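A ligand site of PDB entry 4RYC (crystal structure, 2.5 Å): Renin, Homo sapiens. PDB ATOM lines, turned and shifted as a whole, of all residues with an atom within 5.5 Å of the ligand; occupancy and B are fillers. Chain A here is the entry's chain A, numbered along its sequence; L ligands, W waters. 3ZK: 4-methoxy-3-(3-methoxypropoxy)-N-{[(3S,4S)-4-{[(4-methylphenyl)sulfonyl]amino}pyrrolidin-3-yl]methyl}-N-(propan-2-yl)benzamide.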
ATOM      1  N   THR A  18      34.691  24.078  25.939  1.00  0.00           N
ATOM      2  CA  THR A  18      34.024  22.808  25.680  1.00  0.00           C
ATOM      3  C   THR A  18      33.036  22.895  24.527  1.00  0.00           C
ATOM      4  O   THR A  18      32.786  21.890  23.891  1.00  0.00           O
ATOM      5  CB  THR A  18      33.383  22.205  26.952  1.00  0.00           C
ATOM      6  OG1 THR A  18      32.307  23.015  27.404  1.00  0.00           O
ATOM      7  CG2 THR A  18      34.365  21.985  28.061  1.00  0.00           C
ATOM      8  N   GLN A  19      32.448  24.071  24.260  1.00  0.00           N
ATOM      9  CA  GLN A  19      31.491  24.146  23.150  1.00  0.00           C
ATOM     10  C   GLN A  19      31.807  25.284  22.232  1.00  0.00           C
ATOM     11  O   GLN A  19      31.997  26.406  22.701  1.00  0.00           O
ATOM     12  CB  GLN A  19      30.028  24.210  23.639  1.00  0.00           C
ATOM     13  CG  GLN A  19      29.617  23.051  24.596  1.00  0.00           C
ATOM     14  CD  GLN A  19      28.319  23.319  25.296  1.00  0.00           C
ATOM     15  OE1 GLN A  19      27.376  23.820  24.704  1.00  0.00           O
ATOM     16  NE2 GLN A  19      28.226  22.962  26.578  1.00  0.00           N
ATOM     17  N   TYR A  20      31.870  25.003  20.915  1.00  0.00           N
ATOM     18  CA  TYR A  20      32.123  26.019  19.886  1.00  0.00           C
ATOM     19  C   TYR A  20      30.965  25.963  18.932  1.00  0.00           C
ATOM     20  O   TYR A  20      30.614  24.894  18.432  1.00  0.00           O
ATOM     21  CB  TYR A  20      33.452  25.778  19.143  1.00  0.00           C
ATOM     22  CG  TYR A  20      34.694  25.908  20.010  1.00  0.00           C
ATOM     23  CD1 TYR A  20      35.077  24.874  20.864  1.00  0.00           C
ATOM     24  CD2 TYR A  20      35.484  27.051  19.962  1.00  0.00           C
ATOM     25  CE1 TYR A  20      36.216  24.979  21.655  1.00  0.00           C
ATOM     26  CE2 TYR A  20      36.621  27.168  20.747  1.00  0.00           C
ATOM     27  CZ  TYR A  20      36.982  26.128  21.594  1.00  0.00           C
ATOM     28  OH  TYR A  20      38.116  26.206  22.369  1.00  0.00           O
ATOM     29  N   VAL A  36      26.479  23.930  16.074  1.00  0.00           N
ATOM     30  CA  VAL A  36      27.811  23.335  16.067  1.00  0.00           C
ATOM     31  C   VAL A  36      28.081  22.881  14.612  1.00  0.00           C
ATOM     32  O   VAL A  36      27.248  22.213  13.994  1.00  0.00           O
ATOM     33  CB  VAL A  36      27.847  22.131  17.039  1.00  0.00           C
ATOM     34  CG1 VAL A  36      29.101  21.278  16.839  1.00  0.00           C
ATOM     35  CG2 VAL A  36      27.751  22.614  18.480  1.00  0.00           C
ATOM     36  N   ASP A  38      29.850  20.407  12.739  1.00  0.00           N
ATOM     37  CA  ASP A  38      30.297  19.064  13.159  1.00  0.00           C
ATOM     38  C   ASP A  38      30.770  18.157  12.026  1.00  0.00           C
ATOM     39  O   ASP A  38      29.960  17.702  11.234  1.00  0.00           O
ATOM     40  CB  ASP A  38      29.137  18.434  13.949  1.00  0.00           C
ATOM     41  CG  ASP A  38      29.332  17.050  14.517  1.00  0.00           C
ATOM     42  OD1 ASP A  38      30.481  16.600  14.583  1.00  0.00           O
ATOM     43  OD2 ASP A  38      28.331  16.432  14.920  1.00  0.00           O
ATOM     44  N   GLY A  40      31.941  15.233  12.450  1.00  0.00           N
ATOM     45  CA  GLY A  40      31.570  13.895  12.864  1.00  0.00           C
ATOM     46  C   GLY A  40      30.147  13.506  12.529  1.00  0.00           C
ATOM     47  O   GLY A  40      29.706  12.427  12.919  1.00  0.00           O
ATOM     48  N   SER A  41      29.371  14.391  11.853  1.00  0.00           N
ATOM     49  CA  SER A  41      27.982  14.112  11.473  1.00  0.00           C
ATOM     50  C   SER A  41      27.656  14.779  10.130  1.00  0.00           C
ATOM     51  O   SER A  41      28.402  15.651   9.707  1.00  0.00           O
ATOM     52  CB  SER A  41      26.986  14.457  12.573  1.00  0.00           C
ATOM     53  OG  SER A  41      26.850  15.851  12.789  1.00  0.00           O
ATOM     54  N   TRP A  45      20.264  19.932  11.700  1.00  0.00           N
ATOM     55  CA  TRP A  45      19.090  19.842  12.566  1.00  0.00           C
ATOM     56  C   TRP A  45      19.056  20.943  13.573  1.00  0.00           C
ATOM     57  O   TRP A  45      20.106  21.353  14.061  1.00  0.00           O
ATOM     58  CB  TRP A  45      18.917  18.470  13.229  1.00  0.00           C
ATOM     59  CG  TRP A  45      19.909  18.142  14.309  1.00  0.00           C
ATOM     60  CD1 TRP A  45      21.011  17.355  14.196  1.00  0.00           C
ATOM     61  CD2 TRP A  45      19.799  18.479  15.716  1.00  0.00           C
ATOM     62  NE1 TRP A  45      21.603  17.184  15.426  1.00  0.00           N
ATOM     63  CE2 TRP A  45      20.891  17.887  16.376  1.00  0.00           C
ATOM     64  CE3 TRP A  45      18.892  19.246  16.466  1.00  0.00           C
ATOM     65  CZ2 TRP A  45      21.125  18.058  17.740  1.00  0.00           C
ATOM     66  CZ3 TRP A  45      19.103  19.400  17.821  1.00  0.00           C
ATOM     67  CH2 TRP A  45      20.207  18.815  18.448  1.00  0.00           C
ATOM     68  N   ARG A  82      21.419   9.182  16.173  1.00  0.00           N
ATOM     69  CA  ARG A  82      22.018   8.553  17.329  1.00  0.00           C
ATOM     70  C   ARG A  82      23.459   8.959  17.495  1.00  0.00           C
ATOM     71  O   ARG A  82      24.264   8.739  16.601  1.00  0.00           O
ATOM     72  CB  ARG A  82      21.874   7.021  17.287  1.00  0.00           C
ATOM     73  CG  ARG A  82      20.437   6.546  17.464  1.00  0.00           C
ATOM     74  CD  ARG A  82      20.267   5.085  17.075  1.00  0.00           C
ATOM     75  NE  ARG A  82      18.882   4.648  17.249  1.00  0.00           N
ATOM     76  CZ  ARG A  82      17.993   4.533  16.264  1.00  0.00           C
ATOM     77  NH1 ARG A  82      18.338   4.788  15.011  1.00  0.00           N
ATOM     78  NH2 ARG A  82      16.756   4.143  16.529  1.00  0.00           N
ATOM     79  N   TYR A  83      23.765   9.555  18.640  1.00  0.00           N
ATOM     80  CA  TYR A  83      25.096   9.942  19.020  1.00  0.00           C
ATOM     81  C   TYR A  83      25.486   9.048  20.204  1.00  0.00           C
ATOM     82  O   TYR A  83      24.622   8.476  20.849  1.00  0.00           O
ATOM     83  CB  TYR A  83      25.169  11.447  19.391  1.00  0.00           C
ATOM     84  CG  TYR A  83      24.704  12.373  18.277  1.00  0.00           C
ATOM     85  CD1 TYR A  83      25.307  12.349  17.016  1.00  0.00           C
ATOM     86  CD2 TYR A  83      23.672  13.275  18.487  1.00  0.00           C
ATOM     87  CE1 TYR A  83      24.895  13.197  15.995  1.00  0.00           C
ATOM     88  CE2 TYR A  83      23.239  14.127  17.462  1.00  0.00           C
ATOM     89  CZ  TYR A  83      23.867  14.084  16.222  1.00  0.00           C
ATOM     90  OH  TYR A  83      23.470  14.928  15.218  1.00  0.00           O
ATOM     91  N   SER A  84      26.775   8.948  20.482  1.00  0.00           N
ATOM     92  CA  SER A  84      27.298   8.159  21.606  1.00  0.00           C
ATOM     93  C   SER A  84      26.997   8.879  22.945  1.00  0.00           C
ATOM     94  O   SER A  84      27.275   8.353  24.006  1.00  0.00           O
ATOM     95  CB  SER A  84      28.793   7.940  21.420  1.00  0.00           C
ATOM     96  OG  SER A  84      29.021   7.252  20.192  1.00  0.00           O
ATOM     97  N   THR A  85      26.395  10.066  22.864  1.00  0.00           N
ATOM     98  CA  THR A  85      26.052  10.892  24.029  1.00  0.00           C
ATOM     99  C   THR A  85      24.562  10.959  24.292  1.00  0.00           C
ATOM    100  O   THR A  85      24.148  11.330  25.402  1.00  0.00           O
ATOM    101  CB  THR A  85      26.623  12.300  23.858  1.00  0.00           C
ATOM    102  OG1 THR A  85      26.306  12.765  22.537  1.00  0.00           O
ATOM    103  CG2 THR A  85      28.120  12.346  24.089  1.00  0.00           C
ATOM    104  N   PRO A 118      22.073  14.942  26.747  1.00  0.00           N
ATOM    105  CA  PRO A 118      22.940  16.086  27.115  1.00  0.00           C
ATOM    106  C   PRO A 118      22.468  17.500  26.708  1.00  0.00           C
ATOM    107  O   PRO A 118      23.181  18.463  26.984  1.00  0.00           O
ATOM    108  CB  PRO A 118      24.215  15.745  26.338  1.00  0.00           C
ATOM    109  CG  PRO A 118      23.681  15.156  25.028  1.00  0.00           C
ATOM    110  CD  PRO A 118      22.373  14.466  25.373  1.00  0.00           C
ATOM    111  N   PHE A 119      21.265  17.632  26.120  1.00  0.00           N
ATOM    112  CA  PHE A 119      20.864  18.895  25.488  1.00  0.00           C
ATOM    113  C   PHE A 119      20.503  20.035  26.460  1.00  0.00           C
ATOM    114  O   PHE A 119      20.637  21.180  26.035  1.00  0.00           O
ATOM    115  CB  PHE A 119      19.809  18.677  24.392  1.00  0.00           C
ATOM    116  CG  PHE A 119      20.429  17.807  23.306  1.00  0.00           C
ATOM    117  CD1 PHE A 119      21.457  18.297  22.504  1.00  0.00           C
ATOM    118  CD2 PHE A 119      20.084  16.466  23.182  1.00  0.00           C
ATOM    119  CE1 PHE A 119      22.112  17.458  21.587  1.00  0.00           C
ATOM    120  CE2 PHE A 119      20.741  15.625  22.275  1.00  0.00           C
ATOM    121  CZ  PHE A 119      21.752  16.135  21.482  1.00  0.00           C
ATOM    122  N   LEU A 121      22.513  20.801  28.738  1.00  0.00           N
ATOM    123  CA  LEU A 121      23.873  21.290  28.977  1.00  0.00           C
ATOM    124  C   LEU A 121      24.394  22.018  27.746  1.00  0.00           C
ATOM    125  O   LEU A 121      25.451  22.672  27.794  1.00  0.00           O
ATOM    126  CB  LEU A 121      24.847  20.140  29.335  1.00  0.00           C
ATOM    127  CG  LEU A 121      24.497  19.185  30.498  1.00  0.00           C
ATOM    128  CD1 LEU A 121      25.308  17.918  30.400  1.00  0.00           C
ATOM    129  CD2 LEU A 121      24.712  19.825  31.847  1.00  0.00           C
ATOM    130  N   ALA A 122      23.655  21.890  26.625  1.00  0.00           N
ATOM    131  CA  ALA A 122      24.054  22.522  25.368  1.00  0.00           C
ATOM    132  C   ALA A 122      23.733  24.011  25.378  1.00  0.00           C
ATOM    133  O   ALA A 122      22.618  24.415  25.728  1.00  0.00           O
ATOM    134  CB  ALA A 122      23.391  21.836  24.173  1.00  0.00           C
ATOM    135  N   PHE A 124      24.385  25.521  22.433  1.00  0.00           N
ATOM    136  CA  PHE A 124      23.943  25.572  21.039  1.00  0.00           C
ATOM    137  C   PHE A 124      22.527  25.001  20.953  1.00  0.00           C
ATOM    138  O   PHE A 124      22.138  24.209  21.827  1.00  0.00           O
ATOM    139  CB  PHE A 124      24.912  24.762  20.136  1.00  0.00           C
ATOM    140  CG  PHE A 124      25.141  23.325  20.565  1.00  0.00           C
ATOM    141  CD1 PHE A 124      26.108  23.010  21.506  1.00  0.00           C
ATOM    142  CD2 PHE A 124      24.378  22.282  20.027  1.00  0.00           C
ATOM    143  CE1 PHE A 124      26.311  21.665  21.902  1.00  0.00           C
ATOM    144  CE2 PHE A 124      24.580  20.949  20.415  1.00  0.00           C
ATOM    145  CZ  PHE A 124      25.548  20.654  21.361  1.00  0.00           C
ATOM    146  N   VAL A 127      22.785  21.498  15.092  1.00  0.00           N
ATOM    147  CA  VAL A 127      24.007  21.019  14.442  1.00  0.00           C
ATOM    148  C   VAL A 127      23.950  21.251  12.955  1.00  0.00           C
ATOM    149  O   VAL A 127      22.887  21.119  12.339  1.00  0.00           O
ATOM    150  CB  VAL A 127      24.207  19.494  14.772  1.00  0.00           C
ATOM    151  CG1 VAL A 127      25.438  18.897  14.090  1.00  0.00           C
ATOM    152  CG2 VAL A 127      24.270  19.266  16.280  1.00  0.00           C
ATOM    153  N   GLN A 135      27.361   9.182   5.271  1.00  0.00           N
ATOM    154  CA  GLN A 135      26.953   9.023   6.670  1.00  0.00           C
ATOM    155  C   GLN A 135      25.721   9.845   7.038  1.00  0.00           C
ATOM    156  O   GLN A 135      25.331   9.872   8.203  1.00  0.00           O
ATOM    157  CB  GLN A 135      28.111   9.292   7.637  1.00  0.00           C
ATOM    158  CG  GLN A 135      29.191   8.214   7.593  1.00  0.00           C
ATOM    159  CD  GLN A 135      30.207   8.370   8.705  1.00  0.00           C
ATOM    160  OE1 GLN A 135      30.687   7.378   9.247  1.00  0.00           O
ATOM    161  NE2 GLN A 135      30.562   9.612   9.077  1.00  0.00           N
ATOM    162  N   TYR A 162      39.839  27.005  16.472  1.00  0.00           N
ATOM    163  CA  TYR A 162      39.238  27.031  17.817  1.00  0.00           C
ATOM    164  C   TYR A 162      40.234  27.727  18.741  1.00  0.00           C
ATOM    165  O   TYR A 162      41.321  27.212  18.975  1.00  0.00           O
ATOM    166  CB  TYR A 162      38.925  25.620  18.347  1.00  0.00           C
ATOM    167  CG  TYR A 162      37.690  24.938  17.774  1.00  0.00           C
ATOM    168  CD1 TYR A 162      36.814  25.633  16.937  1.00  0.00           C
ATOM    169  CD2 TYR A 162      37.374  23.632  18.118  1.00  0.00           C
ATOM    170  CE1 TYR A 162      35.678  25.012  16.418  1.00  0.00           C
ATOM    171  CE2 TYR A 162      36.223  23.007  17.623  1.00  0.00           C
ATOM    172  CZ  TYR A 162      35.368  23.710  16.783  1.00  0.00           C
ATOM    173  OH  TYR A 162      34.226  23.107  16.323  1.00  0.00           O
ATOM    174  N   VAL A 200      33.923   9.540   5.383  1.00  0.00           N
ATOM    175  CA  VAL A 200      34.168   9.818   6.814  1.00  0.00           C
ATOM    176  C   VAL A 200      35.455  10.653   6.967  1.00  0.00           C
ATOM    177  O   VAL A 200      36.436  10.380   6.281  1.00  0.00           O
ATOM    178  CB  VAL A 200      34.252   8.536   7.701  1.00  0.00           C
ATOM    179  CG1 VAL A 200      33.994   8.840   9.179  1.00  0.00           C
ATOM    180  CG2 VAL A 200      33.376   7.389   7.217  1.00  0.00           C
ATOM    181  N   LEU A 224      39.293   9.839  14.110  1.00  0.00           N
ATOM    182  CA  LEU A 224      38.217  10.650  13.565  1.00  0.00           C
ATOM    183  C   LEU A 224      38.532  12.107  13.959  1.00  0.00           C
ATOM    184  O   LEU A 224      38.802  12.371  15.125  1.00  0.00           O
ATOM    185  CB  LEU A 224      36.845  10.198  14.113  1.00  0.00           C
ATOM    186  CG  LEU A 224      35.625  11.014  13.648  1.00  0.00           C
ATOM    187  CD1 LEU A 224      35.290  10.741  12.188  1.00  0.00           C
ATOM    188  CD2 LEU A 224      34.440  10.736  14.533  1.00  0.00           C
ATOM    189  N   ASP A 226      37.062  15.209  14.631  1.00  0.00           N
ATOM    190  CA  ASP A 226      35.714  15.620  14.998  1.00  0.00           C
ATOM    191  C   ASP A 226      35.584  17.021  15.638  1.00  0.00           C
ATOM    192  O   ASP A 226      35.767  17.181  16.843  1.00  0.00           O
ATOM    193  CB  ASP A 226      35.098  14.542  15.910  1.00  0.00           C
ATOM    194  CG  ASP A 226      33.607  14.617  16.091  1.00  0.00           C
ATOM    195  OD1 ASP A 226      32.989  15.563  15.539  1.00  0.00           O
ATOM    196  OD2 ASP A 226      33.046  13.735  16.752  1.00  0.00           O
ATOM    197  N   THR A 227      35.171  18.005  14.833  1.00  0.00           N
ATOM    198  CA  THR A 227      34.972  19.402  15.245  1.00  0.00           C
ATOM    199  C   THR A 227      33.789  19.571  16.243  1.00  0.00           C
ATOM    200  O   THR A 227      33.778  20.555  16.992  1.00  0.00           O
ATOM    201  CB  THR A 227      34.820  20.303  14.025  1.00  0.00           C
ATOM    202  OG1 THR A 227      33.661  19.903  13.312  1.00  0.00           O
ATOM    203  CG2 THR A 227      36.051  20.274  13.115  1.00  0.00           C
ATOM    204  N   GLY A 228      32.857  18.619  16.236  1.00  0.00           N
ATOM    205  CA  GLY A 228      31.703  18.613  17.129  1.00  0.00           C
ATOM    206  C   GLY A 228      31.969  17.992  18.476  1.00  0.00           C
ATOM    207  O   GLY A 228      31.069  17.945  19.316  1.00  0.00           O
ATOM    208  N   ALA A 229      33.167  17.460  18.700  1.00  0.00           N
ATOM    209  CA  ALA A 229      33.525  16.839  19.961  1.00  0.00           C
ATOM    210  C   ALA A 229      34.381  17.817  20.789  1.00  0.00           C
ATOM    211  O   ALA A 229      35.212  18.548  20.234  1.00  0.00           O
ATOM    212  CB  ALA A 229      34.310  15.553  19.684  1.00  0.00           C
ATOM    213  N   SER A 230      34.153  17.858  22.098  1.00  0.00           N
ATOM    214  CA  SER A 230      34.865  18.735  23.021  1.00  0.00           C
ATOM    215  C   SER A 230      36.283  18.286  23.285  1.00  0.00           C
ATOM    216  O   SER A 230      37.159  19.127  23.489  1.00  0.00           O
ATOM    217  CB  SER A 230      34.160  18.802  24.361  1.00  0.00           C
ATOM    218  OG  SER A 230      32.824  19.238  24.254  1.00  0.00           O
ATOM    219  N   MET A 303      35.127   7.186  24.864  1.00  0.00           N
ATOM    220  CA  MET A 303      33.972   7.235  23.988  1.00  0.00           C
ATOM    221  C   MET A 303      34.017   6.037  23.038  1.00  0.00           C
ATOM    222  O   MET A 303      34.883   5.952  22.163  1.00  0.00           O
ATOM    223  CB  MET A 303      33.860   8.563  23.226  1.00  0.00           C
ATOM    224  CG  MET A 303      32.588   8.671  22.415  1.00  0.00           C
ATOM    225  SD  MET A 303      31.475   9.994  22.974  1.00  0.00           S
ATOM    226  CE  MET A 303      30.975   9.383  24.633  1.00  0.00           C
ATOM    227  N   ILE A 305      32.741   4.564  20.133  1.00  0.00           N
ATOM    228  CA  ILE A 305      32.047   4.913  18.887  1.00  0.00           C
ATOM    229  C   ILE A 305      31.737   3.581  18.216  1.00  0.00           C
ATOM    230  O   ILE A 305      32.627   2.736  18.130  1.00  0.00           O
ATOM    231  CB  ILE A 305      32.897   5.892  18.051  1.00  0.00           C
ATOM    232  CG1 ILE A 305      33.101   7.218  18.832  1.00  0.00           C
ATOM    233  CG2 ILE A 305      32.292   6.137  16.683  1.00  0.00           C
ATOM    234  CD1 ILE A 305      34.374   7.983  18.621  1.00  0.00           C
ATOM    235  N   PRO A 306      30.448   3.338  17.862  1.00  0.00           N
ATOM    236  CA  PRO A 306      30.091   2.009  17.288  1.00  0.00           C
ATOM    237  C   PRO A 306      30.583   1.753  15.869  1.00  0.00           C
ATOM    238  O   PRO A 306      30.768   2.726  15.144  1.00  0.00           O
ATOM    239  CB  PRO A 306      28.556   2.033  17.307  1.00  0.00           C
ATOM    240  CG  PRO A 306      28.200   3.495  17.181  1.00  0.00           C
ATOM    241  CD  PRO A 306      29.272   4.229  17.956  1.00  0.00           C
ATOM    242  N   THR A 309      32.330   3.061  11.834  1.00  0.00           N
ATOM    243  CA  THR A 309      33.232   4.186  12.178  1.00  0.00           C
ATOM    244  C   THR A 309      34.175   3.788  13.316  1.00  0.00           C
ATOM    245  O   THR A 309      35.381   3.905  13.171  1.00  0.00           O
ATOM    246  CB  THR A 309      32.461   5.499  12.426  1.00  0.00           C
ATOM    247  OG1 THR A 309      31.685   5.783  11.270  1.00  0.00           O
ATOM    248  CG2 THR A 309      33.403   6.705  12.716  1.00  0.00           C
ATOM    249  N   ALA A 317      37.911  19.327  20.061  1.00  0.00           N
ATOM    250  CA  ALA A 317      38.369  20.705  20.336  1.00  0.00           C
ATOM    251  C   ALA A 317      39.727  20.773  21.021  1.00  0.00           C
ATOM    252  O   ALA A 317      40.499  21.683  20.696  1.00  0.00           O
ATOM    253  CB  ALA A 317      37.340  21.493  21.132  1.00  0.00           C
HETATM  254  C2  3ZK L   1      27.625  15.700  20.792  1.00  0.00           C
HETATM  255  C13 3ZK L   1      28.417  18.750  22.943  1.00  0.00           C
HETATM  256  C16 3ZK L   1      27.453  18.632  23.983  1.00  0.00           C
HETATM  257  C17 3ZK L   1      26.578  16.603  22.937  1.00  0.00           C
HETATM  258  C18 3ZK L   1      26.904  17.224  18.969  1.00  0.00           C
HETATM  259  C19 3ZK L   1      26.510  17.572  23.952  1.00  0.00           C
HETATM  260  C20 3ZK L   1      30.962  10.284  15.567  1.00  0.00           C
HETATM  261  C21 3ZK L   1      28.903   9.057  15.954  1.00  0.00           C
HETATM  262  C22 3ZK L   1      30.077  15.167  17.676  1.00  0.00           C
HETATM  263  C23 3ZK L   1      29.422  13.535  16.071  1.00  0.00           C
HETATM  264  C25 3ZK L   1      30.965   9.825  14.241  1.00  0.00           C
HETATM  265  C26 3ZK L   1      28.916   8.598  14.625  1.00  0.00           C
HETATM  266  C27 3ZK L   1      29.953   8.990  13.753  1.00  0.00           C
HETATM  267  C29 3ZK L   1      29.938  21.048  21.018  1.00  0.00           C
HETATM  268  S1  3ZK L   1      29.921  10.436  18.115  1.00  0.00           S
HETATM  269  N3  3ZK L   1      27.451  15.930  19.450  1.00  0.00           N
HETATM  270  N4  3ZK L   1      30.159  12.038  17.950  1.00  0.00           N
HETATM  271  C5  3ZK L   1      27.611  14.794  18.498  1.00  0.00           C
HETATM  272  C6  3ZK L   1      29.054  14.231  18.355  1.00  0.00           C
HETATM  273  C7  3ZK L   1      27.522  16.744  21.898  1.00  0.00           C
HETATM  274  C8  3ZK L   1      29.135  12.952  17.471  1.00  0.00           C
HETATM  275  C9  3ZK L   1      29.921   9.916  16.425  1.00  0.00           C
HETATM  276  C10 3ZK L   1      28.459  17.777  21.912  1.00  0.00           C
HETATM  277  O11 3ZK L   1      31.076   9.869  18.776  1.00  0.00           O
HETATM  278  O12 3ZK L   1      28.659  10.183  18.740  1.00  0.00           O
HETATM  279  N14 3ZK L   1      30.435  14.555  16.382  1.00  0.00           N
HETATM  280  O15 3ZK L   1      27.987  14.625  21.247  1.00  0.00           O
HETATM  281  O24 3ZK L   1      29.311  19.824  23.064  1.00  0.00           O
HETATM  282  O28 3ZK L   1      27.495  19.574  25.026  1.00  0.00           O
HETATM  283  O30 3ZK L   1      32.113  21.969  20.482  1.00  0.00           O
HETATM  284  C31 3ZK L   1      30.400  20.115  22.164  1.00  0.00           C
HETATM  285  C32 3ZK L   1      31.040  21.191  19.950  1.00  0.00           C
HETATM  286  C33 3ZK L   1      27.630  18.067  17.874  1.00  0.00           C
HETATM  287  C34 3ZK L   1      25.378  17.060  18.726  1.00  0.00           C
HETATM  288  C35 3ZK L   1      29.964   8.497  12.300  1.00  0.00           C
HETATM  289  C36 3ZK L   1      26.506  19.612  26.069  1.00  0.00           C
HETATM  290  C37 3ZK L   1      33.406  21.411  20.198  1.00  0.00           C
HETATM  291  O   HOH W   1      30.773  19.291  26.065  1.00  0.00           O
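Water W1 bridges OG of Ser 230 and O24 of the ligand.
OD1 of Asp 38 lies within salt-bridge range of N14 of the ligand (2.7 Å). OD2 of Asp 226 lies within salt-bridge range of N14 of the ligand. The side-chain hydroxyl (OG1) of Thr 85 is in hydrogen-bond range of an oxygen (O15) of the ligand, 2.8 Å away. O12 of the ligand sits at hydrogen-bond distance from N of Ser 84, at 2.8 Å. An oxygen (O12) of the ligand is in hydrogen-bond range of the side-chain hydroxyl (OG) of Ser 84, 3.3 Å away. The backbone NH (N) of Tyr 20 lies within hydrogen-bond range of an oxygen (O30) of the ligand (3.1 Å).
The backbone carbonyl oxygen of Thr 18 sits close to an oxygen (O30) of the ligand (3.5 Å). Merely in contact with the ligand: Gln 19 (3.5 Å), Val 36 (3.7 Å), Gly 40 (3.2 Å), Tyr 83 (3.6 Å), Pro 118 (3.6 Å), Leu 121 (3.6 Å), Ala 122 (3.7 Å), Phe 124 (3.7 Å), Val 127 (3.5 Å), Gln 135 (3.3 Å), Leu 224 (3.6 Å), Thr 227 (3.3 Å), Gly 228 (3.3 Å), Ala 229 (3.4 Å), Ser 230 (3.3 Å), Ile 305 (3.3 Å) and Thr 309 (3.4 Å). Hydrophobic or aromatic side chains within 4 Å of the ligand: Tyr 20, Val 36, Tyr 83, Pro 118, Leu 121, Phe 124, Val 127, Leu 224 and Ile 305. Within 4 Å of the ligand: Thr 18, Gln 19, Tyr 20, Val 36, Asp 38, Gly 40, Tyr 83, Ser 84, Thr 85, Pro 118, Leu 121, Ala 122, Phe 124, Val 127, Gln 135, Leu 224, Asp 226, Thr 227, Gly 228, Ala 229, Ser 230, Ile 305 and Thr 309.
The side-chain carboxylate (OD1) of Asp 38 lies within hydrogen-bond range of the backbone NH (N) of Gly 40 (2.9 Å). OD2 of Asp 38 is in hydrogen-bond range of OG of Ser 41 (2.7 Å). The side-chain carboxylate (OD1) of Asp 226 sits at hydrogen-bond distance from the backbone NH (N) of Gly 40, 3.3 Å away. The backbone NH of Gly 228 sits at hydrogen-bond distance from the side-chain carboxylate of Asp 226, 3.1 Å away. The side-chain hydroxyl (OG) of Ser 230 sits at hydrogen-bond distance from the backbone carbonyl oxygen (O) of Thr 18 (2.7 Å). OH of Tyr 162 lies within hydrogen-bond range of O of Thr 227 (2.7 Å). O of Ala 229 is in hydrogen-bond range of N of Ala 317 (2.8 Å). NE2 of Gln 19 sits at hydrogen-bond distance from O of Leu 121 (3.0 Å).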
